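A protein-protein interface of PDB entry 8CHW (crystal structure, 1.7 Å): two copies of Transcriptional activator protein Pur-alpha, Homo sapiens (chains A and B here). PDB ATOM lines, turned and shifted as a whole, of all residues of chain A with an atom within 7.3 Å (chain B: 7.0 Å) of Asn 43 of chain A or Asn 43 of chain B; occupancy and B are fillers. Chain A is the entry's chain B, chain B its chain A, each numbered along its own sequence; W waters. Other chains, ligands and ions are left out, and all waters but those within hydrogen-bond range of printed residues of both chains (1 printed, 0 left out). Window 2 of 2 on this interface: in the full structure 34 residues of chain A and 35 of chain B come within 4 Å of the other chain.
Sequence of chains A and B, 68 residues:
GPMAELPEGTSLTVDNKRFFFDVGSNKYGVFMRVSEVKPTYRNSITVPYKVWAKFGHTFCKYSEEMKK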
ATOM      1  N   ARG A  18      28.245 -29.934  -4.622  1.00  0.00           N
ATOM      2  CA  ARG A  18      27.426 -30.942  -5.313  1.00  0.00           C
ATOM      3  C   ARG A  18      26.011 -30.416  -5.539  1.00  0.00           C
ATOM      4  O   ARG A  18      25.384 -29.869  -4.583  1.00  0.00           O
ATOM      5  CB  ARG A  18      27.411 -32.257  -4.527  1.00  0.00           C
ATOM      6  CG  ARG A  18      26.811 -33.402  -5.316  1.00  0.00           C
ATOM      7  CD  ARG A  18      27.247 -34.742  -4.715  1.00  0.00           C
ATOM      8  NE  ARG A  18      26.734 -35.813  -5.539  1.00  0.00           N
ATOM      9  CZ  ARG A  18      26.635 -37.086  -5.163  1.00  0.00           C
ATOM     10  NH1 ARG A  18      26.110 -37.959  -5.997  1.00  0.00           N
ATOM     11  NH2 ARG A  18      26.987 -37.450  -3.949  1.00  0.00           N
ATOM     12  N   PHE A  19      25.530 -30.637  -6.762  1.00  0.00           N
ATOM     13  CA  PHE A  19      24.160 -30.280  -7.177  1.00  0.00           C
ATOM     14  C   PHE A  19      23.342 -31.556  -7.293  1.00  0.00           C
ATOM     15  O   PHE A  19      23.811 -32.470  -7.925  1.00  0.00           O
ATOM     16  CB  PHE A  19      24.177 -29.494  -8.480  1.00  0.00           C
ATOM     17  CG  PHE A  19      24.970 -28.220  -8.372  1.00  0.00           C
ATOM     18  CD1 PHE A  19      24.392 -27.062  -7.868  1.00  0.00           C
ATOM     19  CD2 PHE A  19      26.277 -28.169  -8.838  1.00  0.00           C
ATOM     20  CE1 PHE A  19      25.137 -25.890  -7.774  1.00  0.00           C
ATOM     21  CE2 PHE A  19      27.009 -26.999  -8.739  1.00  0.00           C
ATOM     22  CZ  PHE A  19      26.439 -25.860  -8.207  1.00  0.00           C
ATOM     23  N   PHE A  20      22.201 -31.600  -6.628  1.00  0.00           N
ATOM     24  CA  PHE A  20      21.238 -32.718  -6.760  1.00  0.00           C
ATOM     25  C   PHE A  20      19.983 -32.215  -7.466  1.00  0.00           C
ATOM     26  O   PHE A  20      19.421 -31.190  -7.037  1.00  0.00           O
ATOM     27  CB  PHE A  20      20.894 -33.304  -5.393  1.00  0.00           C
ATOM     28  CG  PHE A  20      22.049 -33.998  -4.708  1.00  0.00           C
ATOM     29  CD1 PHE A  20      22.328 -35.329  -4.966  1.00  0.00           C
ATOM     30  CD2 PHE A  20      22.865 -33.313  -3.825  1.00  0.00           C
ATOM     31  CE1 PHE A  20      23.373 -35.973  -4.318  1.00  0.00           C
ATOM     32  CE2 PHE A  20      23.923 -33.949  -3.198  1.00  0.00           C
ATOM     33  CZ  PHE A  20      24.164 -35.280  -3.432  1.00  0.00           C
ATOM     34  N   ARG A  33      13.420 -30.051  -7.586  1.00  0.00           N
ATOM     35  CA  ARG A  33      14.284 -29.441  -6.568  1.00  0.00           C
ATOM     36  C   ARG A  33      15.723 -29.524  -7.082  1.00  0.00           C
ATOM     37  O   ARG A  33      16.205 -30.607  -7.430  1.00  0.00           O
ATOM     38  CB  ARG A  33      14.087 -30.097  -5.206  1.00  0.00           C
ATOM     39  CG  ARG A  33      14.834 -29.370  -4.097  1.00  0.00           C
ATOM     40  CD  ARG A  33      14.659 -30.100  -2.800  1.00  0.00           C
ATOM     41  NE  ARG A  33      13.223 -30.140  -2.573  1.00  0.00           N
ATOM     42  CZ  ARG A  33      12.499 -29.160  -2.050  1.00  0.00           C
ATOM     43  NH1 ARG A  33      13.079 -28.027  -1.677  1.00  0.00           N
ATOM     44  NH2 ARG A  33      11.191 -29.330  -1.880  1.00  0.00           N
ATOM     45  N   VAL A  34      16.374 -28.372  -7.175  1.00  0.00           N
ATOM     46  CA  VAL A  34      17.828 -28.290  -7.434  1.00  0.00           C
ATOM     47  C   VAL A  34      18.486 -27.839  -6.142  1.00  0.00           C
ATOM     48  O   VAL A  34      18.244 -26.684  -5.691  1.00  0.00           O
ATOM     49  CB  VAL A  34      18.133 -27.341  -8.602  1.00  0.00           C
ATOM     50  CG1 VAL A  34      19.590 -27.403  -8.989  1.00  0.00           C
ATOM     51  CG2 VAL A  34      17.198 -27.650  -9.764  1.00  0.00           C
ATOM     52  N   SER A  35      19.237 -28.747  -5.548  1.00  0.00           N
ATOM     53  CA  SER A  35      19.873 -28.530  -4.237  1.00  0.00           C
ATOM     54  C   SER A  35      21.361 -28.307  -4.487  1.00  0.00           C
ATOM     55  O   SER A  35      21.946 -29.016  -5.317  1.00  0.00           O
ATOM     56  CB  SER A  35      19.645 -29.711  -3.312  1.00  0.00           C
ATOM     57  OG  SER A  35      18.274 -29.910  -3.058  1.00  0.00           O
ATOM     58  N   GLU A  36      21.958 -27.373  -3.785  1.00  0.00           N
ATOM     59  CA  GLU A  36      23.436 -27.267  -3.741  1.00  0.00           C
ATOM     60  C   GLU A  36      23.853 -27.649  -2.314  1.00  0.00           C
ATOM     61  O   GLU A  36      23.190 -27.199  -1.348  1.00  0.00           O
ATOM     62  CB  GLU A  36      23.928 -25.897  -4.212  1.00  0.00           C
ATOM     63  CG  GLU A  36      23.515 -24.769  -3.310  1.00  0.00           C
ATOM     64  CD  GLU A  36      24.004 -23.396  -3.744  1.00  0.00           C
ATOM     65  OE1 GLU A  36      23.798 -22.450  -2.998  1.00  0.00           O
ATOM     66  OE2 GLU A  36      24.545 -23.282  -4.841  1.00  0.00           O
ATOM     67  N   VAL A  37      24.859 -28.513  -2.221  1.00  0.00           N
ATOM     68  CA  VAL A  37      25.388 -29.075  -0.948  1.00  0.00           C
ATOM     69  C   VAL A  37      26.899 -28.817  -0.886  1.00  0.00           C
ATOM     70  O   VAL A  37      27.630 -29.135  -1.849  1.00  0.00           O
ATOM     71  CB  VAL A  37      25.043 -30.566  -0.800  1.00  0.00           C
ATOM     72  CG1 VAL A  37      25.453 -31.102   0.573  1.00  0.00           C
ATOM     73  CG2 VAL A  37      23.570 -30.835  -1.045  1.00  0.00           C
ATOM     74  N   LYS A  38      27.325 -28.197   0.213  1.00  0.00           N
ATOM     75  CA  LYS A  38      28.741 -27.999   0.627  1.00  0.00           C
ATOM     76  C   LYS A  38      28.878 -28.548   2.046  1.00  0.00           C
ATOM     77  O   LYS A  38      27.864 -28.749   2.720  1.00  0.00           O
ATOM     78  CB  LYS A  38      29.111 -26.513   0.581  1.00  0.00           C
ATOM     79  CG  LYS A  38      29.285 -25.911  -0.807  1.00  0.00           C
ATOM     80  CD  LYS A  38      29.731 -24.459  -0.785  1.00  0.00           C
ATOM     81  CE  LYS A  38      28.694 -23.539  -0.167  1.00  0.00           C
ATOM     82  NZ  LYS A  38      29.185 -22.149   0.000  1.00  0.00           N
ATOM     83  N   TYR A  41      26.544 -26.766   4.617  1.00  0.00           N
ATOM     84  CA  TYR A  41      25.559 -25.930   3.870  1.00  0.00           C
ATOM     85  C   TYR A  41      24.772 -26.798   2.874  1.00  0.00           C
ATOM     86  O   TYR A  41      25.393 -27.538   2.076  1.00  0.00           O
ATOM     87  CB  TYR A  41      26.305 -24.751   3.229  1.00  0.00           C
ATOM     88  CG  TYR A  41      25.536 -23.934   2.221  1.00  0.00           C
ATOM     89  CD1 TYR A  41      24.684 -22.913   2.615  1.00  0.00           C
ATOM     90  CD2 TYR A  41      25.677 -24.165   0.861  1.00  0.00           C
ATOM     91  CE1 TYR A  41      23.985 -22.155   1.687  1.00  0.00           C
ATOM     92  CE2 TYR A  41      24.989 -23.415  -0.080  1.00  0.00           C
ATOM     93  CZ  TYR A  41      24.136 -22.406   0.331  1.00  0.00           C
ATOM     94  OH  TYR A  41      23.446 -21.673  -0.596  1.00  0.00           O
ATOM     95  N   ARG A  42      23.438 -26.734   2.948  1.00  0.00           N
ATOM     96  CA  ARG A  42      22.503 -27.320   1.948  1.00  0.00           C
ATOM     97  C   ARG A  42      21.445 -26.263   1.613  1.00  0.00           C
ATOM     98  O   ARG A  42      20.839 -25.720   2.551  1.00  0.00           O
ATOM     99  CB  ARG A  42      21.883 -28.615   2.481  1.00  0.00           C
ATOM    100  CG  ARG A  42      20.711 -29.148   1.663  1.00  0.00           C
ATOM    101  CD  ARG A  42      20.593 -30.665   1.676  1.00  0.00           C
ATOM    102  NE  ARG A  42      19.815 -31.154   0.537  1.00  0.00           N
ATOM    103  CZ  ARG A  42      19.913 -32.381   0.001  1.00  0.00           C
ATOM    104  NH1 ARG A  42      20.747 -33.279   0.497  1.00  0.00           N
ATOM    105  NH2 ARG A  42      19.162 -32.710  -1.032  1.00  0.00           N
ATOM    106  N   ASN A  43      21.227 -25.986   0.325  1.00  0.00           N
ATOM    107  CA  ASN A  43      20.265 -24.953  -0.147  1.00  0.00           C
ATOM    108  C   ASN A  43      19.625 -25.396  -1.469  1.00  0.00           C
ATOM    109  O   ASN A  43      20.284 -26.145  -2.214  1.00  0.00           O
ATOM    110  CB  ASN A  43      20.993 -23.628  -0.319  1.00  0.00           C
ATOM    111  CG  ASN A  43      20.032 -22.496  -0.544  1.00  0.00           C
ATOM    112  OD1 ASN A  43      18.884 -22.557  -0.082  1.00  0.00           O
ATOM    113  ND2 ASN A  43      20.506 -21.468  -1.224  1.00  0.00           N
ATOM    114  N   SER A  44      18.394 -24.967  -1.755  1.00  0.00           N
ATOM    115  CA  SER A  44      17.641 -25.515  -2.911  1.00  0.00           C
ATOM    116  C   SER A  44      16.620 -24.515  -3.437  1.00  0.00           C
ATOM    117  O   SER A  44      16.074 -23.700  -2.671  1.00  0.00           O
ATOM    118  CB  SER A  44      17.007 -26.851  -2.576  1.00  0.00           C
ATOM    119  OG  SER A  44      15.872 -26.646  -1.781  1.00  0.00           O
ATOM    120  N   ILE A  45      16.366 -24.603  -4.729  1.00  0.00           N
ATOM    121  CA  ILE A  45      15.214 -23.906  -5.373  1.00  0.00           C
ATOM    122  C   ILE A  45      14.290 -24.998  -5.927  1.00  0.00           C
ATOM    123  O   ILE A  45      14.752 -26.150  -6.094  1.00  0.00           O
ATOM    124  CB  ILE A  45      15.682 -22.932  -6.468  1.00  0.00           C
ATOM    125  CG1 ILE A  45      16.458 -23.672  -7.564  1.00  0.00           C
ATOM    126  CG2 ILE A  45      16.473 -21.779  -5.875  1.00  0.00           C
ATOM    127  CD1 ILE A  45      16.639 -22.852  -8.821  1.00  0.00           C
ATOM    128  N   ARG B  18       8.746 -16.168  -9.696  1.00  0.00           N
ATOM    129  CA  ARG B  18       9.642 -15.655 -10.754  1.00  0.00           C
ATOM    130  C   ARG B  18      11.067 -16.184 -10.550  1.00  0.00           C
ATOM    131  O   ARG B  18      11.549 -16.112  -9.425  1.00  0.00           O
ATOM    132  CB  ARG B  18       9.618 -14.133 -10.801  1.00  0.00           C
ATOM    133  CG  ARG B  18      10.297 -13.578 -12.038  1.00  0.00           C
ATOM    134  CD  ARG B  18       9.910 -12.111 -12.233  1.00  0.00           C
ATOM    135  NE  ARG B  18      10.586 -11.574 -13.401  1.00  0.00           N
ATOM    136  CZ  ARG B  18      10.685 -10.267 -13.722  1.00  0.00           C
ATOM    137  NH1 ARG B  18      11.335  -9.913 -14.812  1.00  0.00           N
ATOM    138  NH2 ARG B  18      10.141  -9.331 -12.967  1.00  0.00           N
ATOM    139  N   ARG B  33      23.845 -17.147 -10.916  1.00  0.00           N
ATOM    140  CA  ARG B  33      22.912 -17.180  -9.777  1.00  0.00           C
ATOM    141  C   ARG B  33      21.515 -17.464 -10.318  1.00  0.00           C
ATOM    142  O   ARG B  33      21.031 -16.701 -11.194  1.00  0.00           O
ATOM    143  CB  ARG B  33      22.964 -15.894  -8.957  1.00  0.00           C
ATOM    144  CG  ARG B  33      22.055 -15.986  -7.741  1.00  0.00           C
ATOM    145  CD  ARG B  33      22.060 -14.757  -6.840  1.00  0.00           C
ATOM    146  NE  ARG B  33      23.364 -14.422  -6.303  1.00  0.00           N
ATOM    147  CZ  ARG B  33      23.962 -15.011  -5.260  1.00  0.00           C
ATOM    148  NH1 ARG B  33      23.382 -16.000  -4.594  1.00  0.00           N
ATOM    149  NH2 ARG B  33      25.166 -14.607  -4.894  1.00  0.00           N
ATOM    150  N   VAL B  34      20.870 -18.525  -9.844  1.00  0.00           N
ATOM    151  CA  VAL B  34      19.444 -18.797 -10.155  1.00  0.00           C
ATOM    152  C   VAL B  34      18.613 -18.478  -8.919  1.00  0.00           C
ATOM    153  O   VAL B  34      18.738 -19.200  -7.914  1.00  0.00           O
ATOM    154  CB  VAL B  34      19.202 -20.233 -10.654  1.00  0.00           C
ATOM    155  CG1 VAL B  34      17.742 -20.384 -11.104  1.00  0.00           C
ATOM    156  CG2 VAL B  34      20.161 -20.566 -11.795  1.00  0.00           C
ATOM    157  N   SER B  35      17.836 -17.409  -8.991  1.00  0.00           N
ATOM    158  CA  SER B  35      17.021 -16.896  -7.849  1.00  0.00           C
ATOM    159  C   SER B  35      15.565 -17.312  -8.066  1.00  0.00           C
ATOM    160  O   SER B  35      15.045 -17.191  -9.186  1.00  0.00           O
ATOM    161  CB  SER B  35      17.143 -15.394  -7.694  1.00  0.00           C
ATOM    162  OG  SER B  35      18.483 -14.956  -7.446  1.00  0.00           O
ATOM    163  N   GLU B  36      14.897 -17.777  -7.029  1.00  0.00           N
ATOM    164  CA  GLU B  36      13.451 -18.029  -7.102  1.00  0.00           C
ATOM    165  C   GLU B  36      12.810 -16.967  -6.223  1.00  0.00           C
ATOM    166  O   GLU B  36      13.291 -16.789  -5.059  1.00  0.00           O
ATOM    167  CB  GLU B  36      13.176 -19.489  -6.747  1.00  0.00           C
ATOM    168  CG  GLU B  36      12.946 -19.765  -5.286  1.00  0.00           C
ATOM    169  CD  GLU B  36      12.741 -21.242  -4.950  1.00  0.00           C
ATOM    170  OE1 GLU B  36      13.156 -21.659  -3.873  1.00  0.00           O
ATOM    171  OE2 GLU B  36      12.195 -21.943  -5.769  1.00  0.00           O
ATOM    172  N   VAL B  37      11.823 -16.239  -6.754  1.00  0.00           N
ATOM    173  CA  VAL B  37      11.208 -15.100  -6.007  1.00  0.00           C
ATOM    174  C   VAL B  37       9.682 -15.268  -5.938  1.00  0.00           C
ATOM    175  O   VAL B  37       9.043 -15.508  -6.975  1.00  0.00           O
ATOM    176  CB  VAL B  37      11.612 -13.749  -6.614  1.00  0.00           C
ATOM    177  CG1 VAL B  37      10.952 -12.580  -5.879  1.00  0.00           C
ATOM    178  CG2 VAL B  37      13.127 -13.610  -6.644  1.00  0.00           C
ATOM    179  N   LYS B  38       9.131 -15.116  -4.736  1.00  0.00           N
ATOM    180  CA  LYS B  38       7.673 -15.018  -4.469  1.00  0.00           C
ATOM    181  C   LYS B  38       7.444 -13.706  -3.732  1.00  0.00           C
ATOM    182  O   LYS B  38       8.409 -13.080  -3.275  1.00  0.00           O
ATOM    183  CB  LYS B  38       7.198 -16.244  -3.691  1.00  0.00           C
ATOM    184  CG  LYS B  38       7.421 -17.566  -4.412  1.00  0.00           C
ATOM    185  CD  LYS B  38       6.803 -18.762  -3.723  1.00  0.00           C
ATOM    186  CE  LYS B  38       5.348 -18.965  -4.089  1.00  0.00           C
ATOM    187  NZ  LYS B  38       4.743 -20.095  -3.348  1.00  0.00           N
ATOM    188  N   TYR B  41       9.234 -14.060  -0.507  1.00  0.00           N
ATOM    189  CA  TYR B  41      10.242 -15.151  -0.445  1.00  0.00           C
ATOM    190  C   TYR B  41      11.279 -14.949  -1.556  1.00  0.00           C
ATOM    191  O   TYR B  41      10.864 -14.599  -2.660  1.00  0.00           O
ATOM    192  CB  TYR B  41       9.563 -16.510  -0.585  1.00  0.00           C
ATOM    193  CG  TYR B  41      10.536 -17.658  -0.672  1.00  0.00           C
ATOM    194  CD1 TYR B  41      11.101 -18.178   0.473  1.00  0.00           C
ATOM    195  CD2 TYR B  41      10.905 -18.220  -1.891  1.00  0.00           C
ATOM    196  CE1 TYR B  41      12.029 -19.205   0.426  1.00  0.00           C
ATOM    197  CE2 TYR B  41      11.824 -19.260  -1.956  1.00  0.00           C
ATOM    198  CZ  TYR B  41      12.384 -19.761  -0.790  1.00  0.00           C
ATOM    199  OH  TYR B  41      13.319 -20.761  -0.794  1.00  0.00           O
ATOM    200  N   ARG B  42      12.573 -15.112  -1.252  1.00  0.00           N
ATOM    201  CA  ARG B  42      13.667 -15.043  -2.253  1.00  0.00           C
ATOM    202  C   ARG B  42      14.811 -15.955  -1.800  1.00  0.00           C
ATOM    203  O   ARG B  42      15.341 -15.776  -0.696  1.00  0.00           O
ATOM    204  CB  ARG B  42      14.190 -13.616  -2.435  1.00  0.00           C
ATOM    205  CG  ARG B  42      15.460 -13.513  -3.275  1.00  0.00           C
ATOM    206  CD  ARG B  42      15.581 -12.126  -3.913  1.00  0.00           C
ATOM    207  NE  ARG B  42      16.544 -12.200  -5.007  1.00  0.00           N
ATOM    208  CZ  ARG B  42      16.522 -11.476  -6.122  1.00  0.00           C
ATOM    209  NH1 ARG B  42      15.583 -10.578  -6.332  1.00  0.00           N
ATOM    210  NH2 ARG B  42      17.474 -11.653  -7.021  1.00  0.00           N
ATOM    211  N   ASN B  43      15.239 -16.851  -2.675  1.00  0.00           N
ATOM    212  CA  ASN B  43      16.388 -17.745  -2.399  1.00  0.00           C
ATOM    213  C   ASN B  43      17.072 -18.062  -3.730  1.00  0.00           C
ATOM    214  O   ASN B  43      16.457 -17.833  -4.786  1.00  0.00           O
ATOM    215  CB  ASN B  43      15.934 -19.027  -1.704  1.00  0.00           C
ATOM    216  CG  ASN B  43      17.082 -19.836  -1.133  1.00  0.00           C
ATOM    217  OD1 ASN B  43      18.182 -19.333  -0.914  1.00  0.00           O
ATOM    218  ND2 ASN B  43      16.845 -21.118  -0.944  1.00  0.00           N
ATOM    219  N   SER B  44      18.308 -18.539  -3.674  1.00  0.00           N
ATOM    220  CA  SER B  44      19.103 -18.751  -4.908  1.00  0.00           C
ATOM    221  C   SER B  44      20.097 -19.868  -4.682  1.00  0.00           C
ATOM    222  O   SER B  44      20.479 -20.135  -3.522  1.00  0.00           O
ATOM    223  CB  SER B  44      19.748 -17.478  -5.360  1.00  0.00           C
ATOM    224  OG  SER B  44      20.785 -17.094  -4.489  1.00  0.00           O
ATOM    225  N   ILE B  45      20.495 -20.475  -5.791  1.00  0.00           N
ATOM    226  CA  ILE B  45      21.706 -21.329  -5.875  1.00  0.00           C
ATOM    227  C   ILE B  45      22.678 -20.657  -6.839  1.00  0.00           C
ATOM    228  O   ILE B  45      22.255 -19.747  -7.580  1.00  0.00           O
ATOM    229  CB  ILE B  45      21.344 -22.745  -6.331  1.00  0.00           C
ATOM    230  CG1 ILE B  45      20.707 -22.732  -7.722  1.00  0.00           C
ATOM    231  CG2 ILE B  45      20.495 -23.434  -5.294  1.00  0.00           C
ATOM    232  CD1 ILE B  45      20.590 -24.104  -8.318  1.00  0.00           C
ATOM    233  N   THR B  46      23.948 -21.029  -6.770  1.00  0.00           N
ATOM    234  CA  THR B  46      25.012 -20.500  -7.642  1.00  0.00           C
ATOM    235  C   THR B  46      25.708 -21.678  -8.323  1.00  0.00           C
ATOM    236  O   THR B  46      26.002 -22.698  -7.659  1.00  0.00           O
ATOM    237  CB  THR B  46      25.966 -19.558  -6.885  1.00  0.00           C
ATOM    238  OG1 THR B  46      26.500 -20.256  -5.748  1.00  0.00           O
ATOM    239  CG2 THR B  46      25.235 -18.289  -6.477  1.00  0.00           C
HETATM  240  O   HOH W   1      25.018 -20.218  -3.547  1.00  0.00           O
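The side-chain amide nitrogen (ND2) of Asn 43 of chain B lies within hydrogen-bond range of the side-chain amide oxygen (OD1) of Asn 43 of chain A (2.6 Å). O of Ser 44 of chain A lies within hydrogen-bond range of ND2 of Asn 43 of chain B, at 3.2 Å. The backbone carbonyl oxygen (O) of Ser 44 of chain B lies within hydrogen-bond range of the side-chain amide nitrogen (ND2) of Asn 43 of chain A. The backbone NH (N) of Thr 46 of chain B sits at hydrogen-bond distance from the side-chain carboxylate (OE2) of Glu 36 of chain A (3.0 Å).
OG of Ser 44 of chain B is in hydrogen-bond range of NH1 of Arg 33 of chain B, 2.8 Å away. O of Ile 45 of chain B lies within hydrogen-bond range of N of Val 34 of chain B. NH1 of Arg 33 of chain A is in hydrogen-bond range of OG of Ser 44 of chain A (3.1 Å). The backbone NH of Val 34 of chain A is in hydrogen-bond range of the backbone carbonyl oxygen of Ile 45 of chain A (3.0 Å). OE1 of Glu 36 of chain A is in hydrogen-bond range of OH of Tyr 41 of chain A, at 2.5 Å. The backbone NH (N) of Glu 36 of chain A sits at hydrogen-bond distance from the backbone carbonyl oxygen (O) of Asn 43 of chain A (2.6 Å).
Thr 46 of chain B touches Phe 19 of chain A. CG1 of Val 34 of chain A touches CD1 of Ile 45 of chain B, 3.5 Å away. Glu 36 of chain A touches Ile 45 of chain B (OE2 to CB, 3.6 Å). Ser 44 of chain A touches Glu 36 of chain B. Ile 45 of chain A touches Val 34 of chain B (CD1 to CG1, 3.5 Å). Ile 45 of chain A touches Glu 36 of chain B.
Asn 43 of chain A touches just these residues of chain B: Asn 43 (2.6 Å) and Ser 44 (2.7 Å). Of chain A, only Asn 43 (2.6 Å) and Ser 44 (3.2 Å) come within 4 Å of Asn 43 of chain B. Printed residues of chain B within 4 Å of Phe 19 of chain A: Thr 46 (3.2 Å). Of the printed residues of chain B, Val 34 of chain A touches Ile 45 (3.5 Å). Ser 35 of chain B touches none of the printed residues of chain A. Arg 33 of chain A touches none of the printed residues of chain B. The nearest residue of chain B that does not touch Asn 43 of chain A is Ile 45 of chain B (4.1 Å). The nearest residue of chain A that does not touch Asn 43 of chain B is Ile 45 of chain A (4.1 Å).
Of the 13 printed residues of chain B, 6 touch a printed residue of chain A. Hydrophobic or aromatic side chains of chain B that line the printed part of chain A: Val 34 and Ile 45. Of the 14 printed residues of chain A, 6 touch a printed residue of chain B. Printed residues of chain A that touch a printed residue of chain B: Phe 19, Val 34, Glu 36, Asn 43, Ser 44 and Ile 45. Hydrophobic or aromatic side chains of chain A that line the printed part of chain B: Phe 19, Val 34 and Ile 45. Along chain A the printed residues that touch a printed residue of chain B span positions 19 to 45. Among the printed residues, no Asp or Glu carboxylate lies within 4 Å of a Lys or Arg side-chain nitrogen of the other chain.
Val 34 of chain A touches Ile 45 of chain B, and with the chains exchanged Ile 45 of chain A touches Val 34 of chain B. Glu 36 of chain A touches Ile 45 of chain B, and with the chains exchanged Ile 45 of chain A touches Glu 36 of chain B. Asn 43 of chain B touches its own counterpart, Asn 43 of chain A. Asn 43 of chain A touches Ser 44 of chain B, and with the chains exchanged Ser 44 of chain A touches Asn 43 of chain B.
Water W1 lies within hydrogen-bond range of OE1 of Glu 36 of chain A (2.6 Å) and OG1 of Thr 46 of chain B (2.7 Å).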
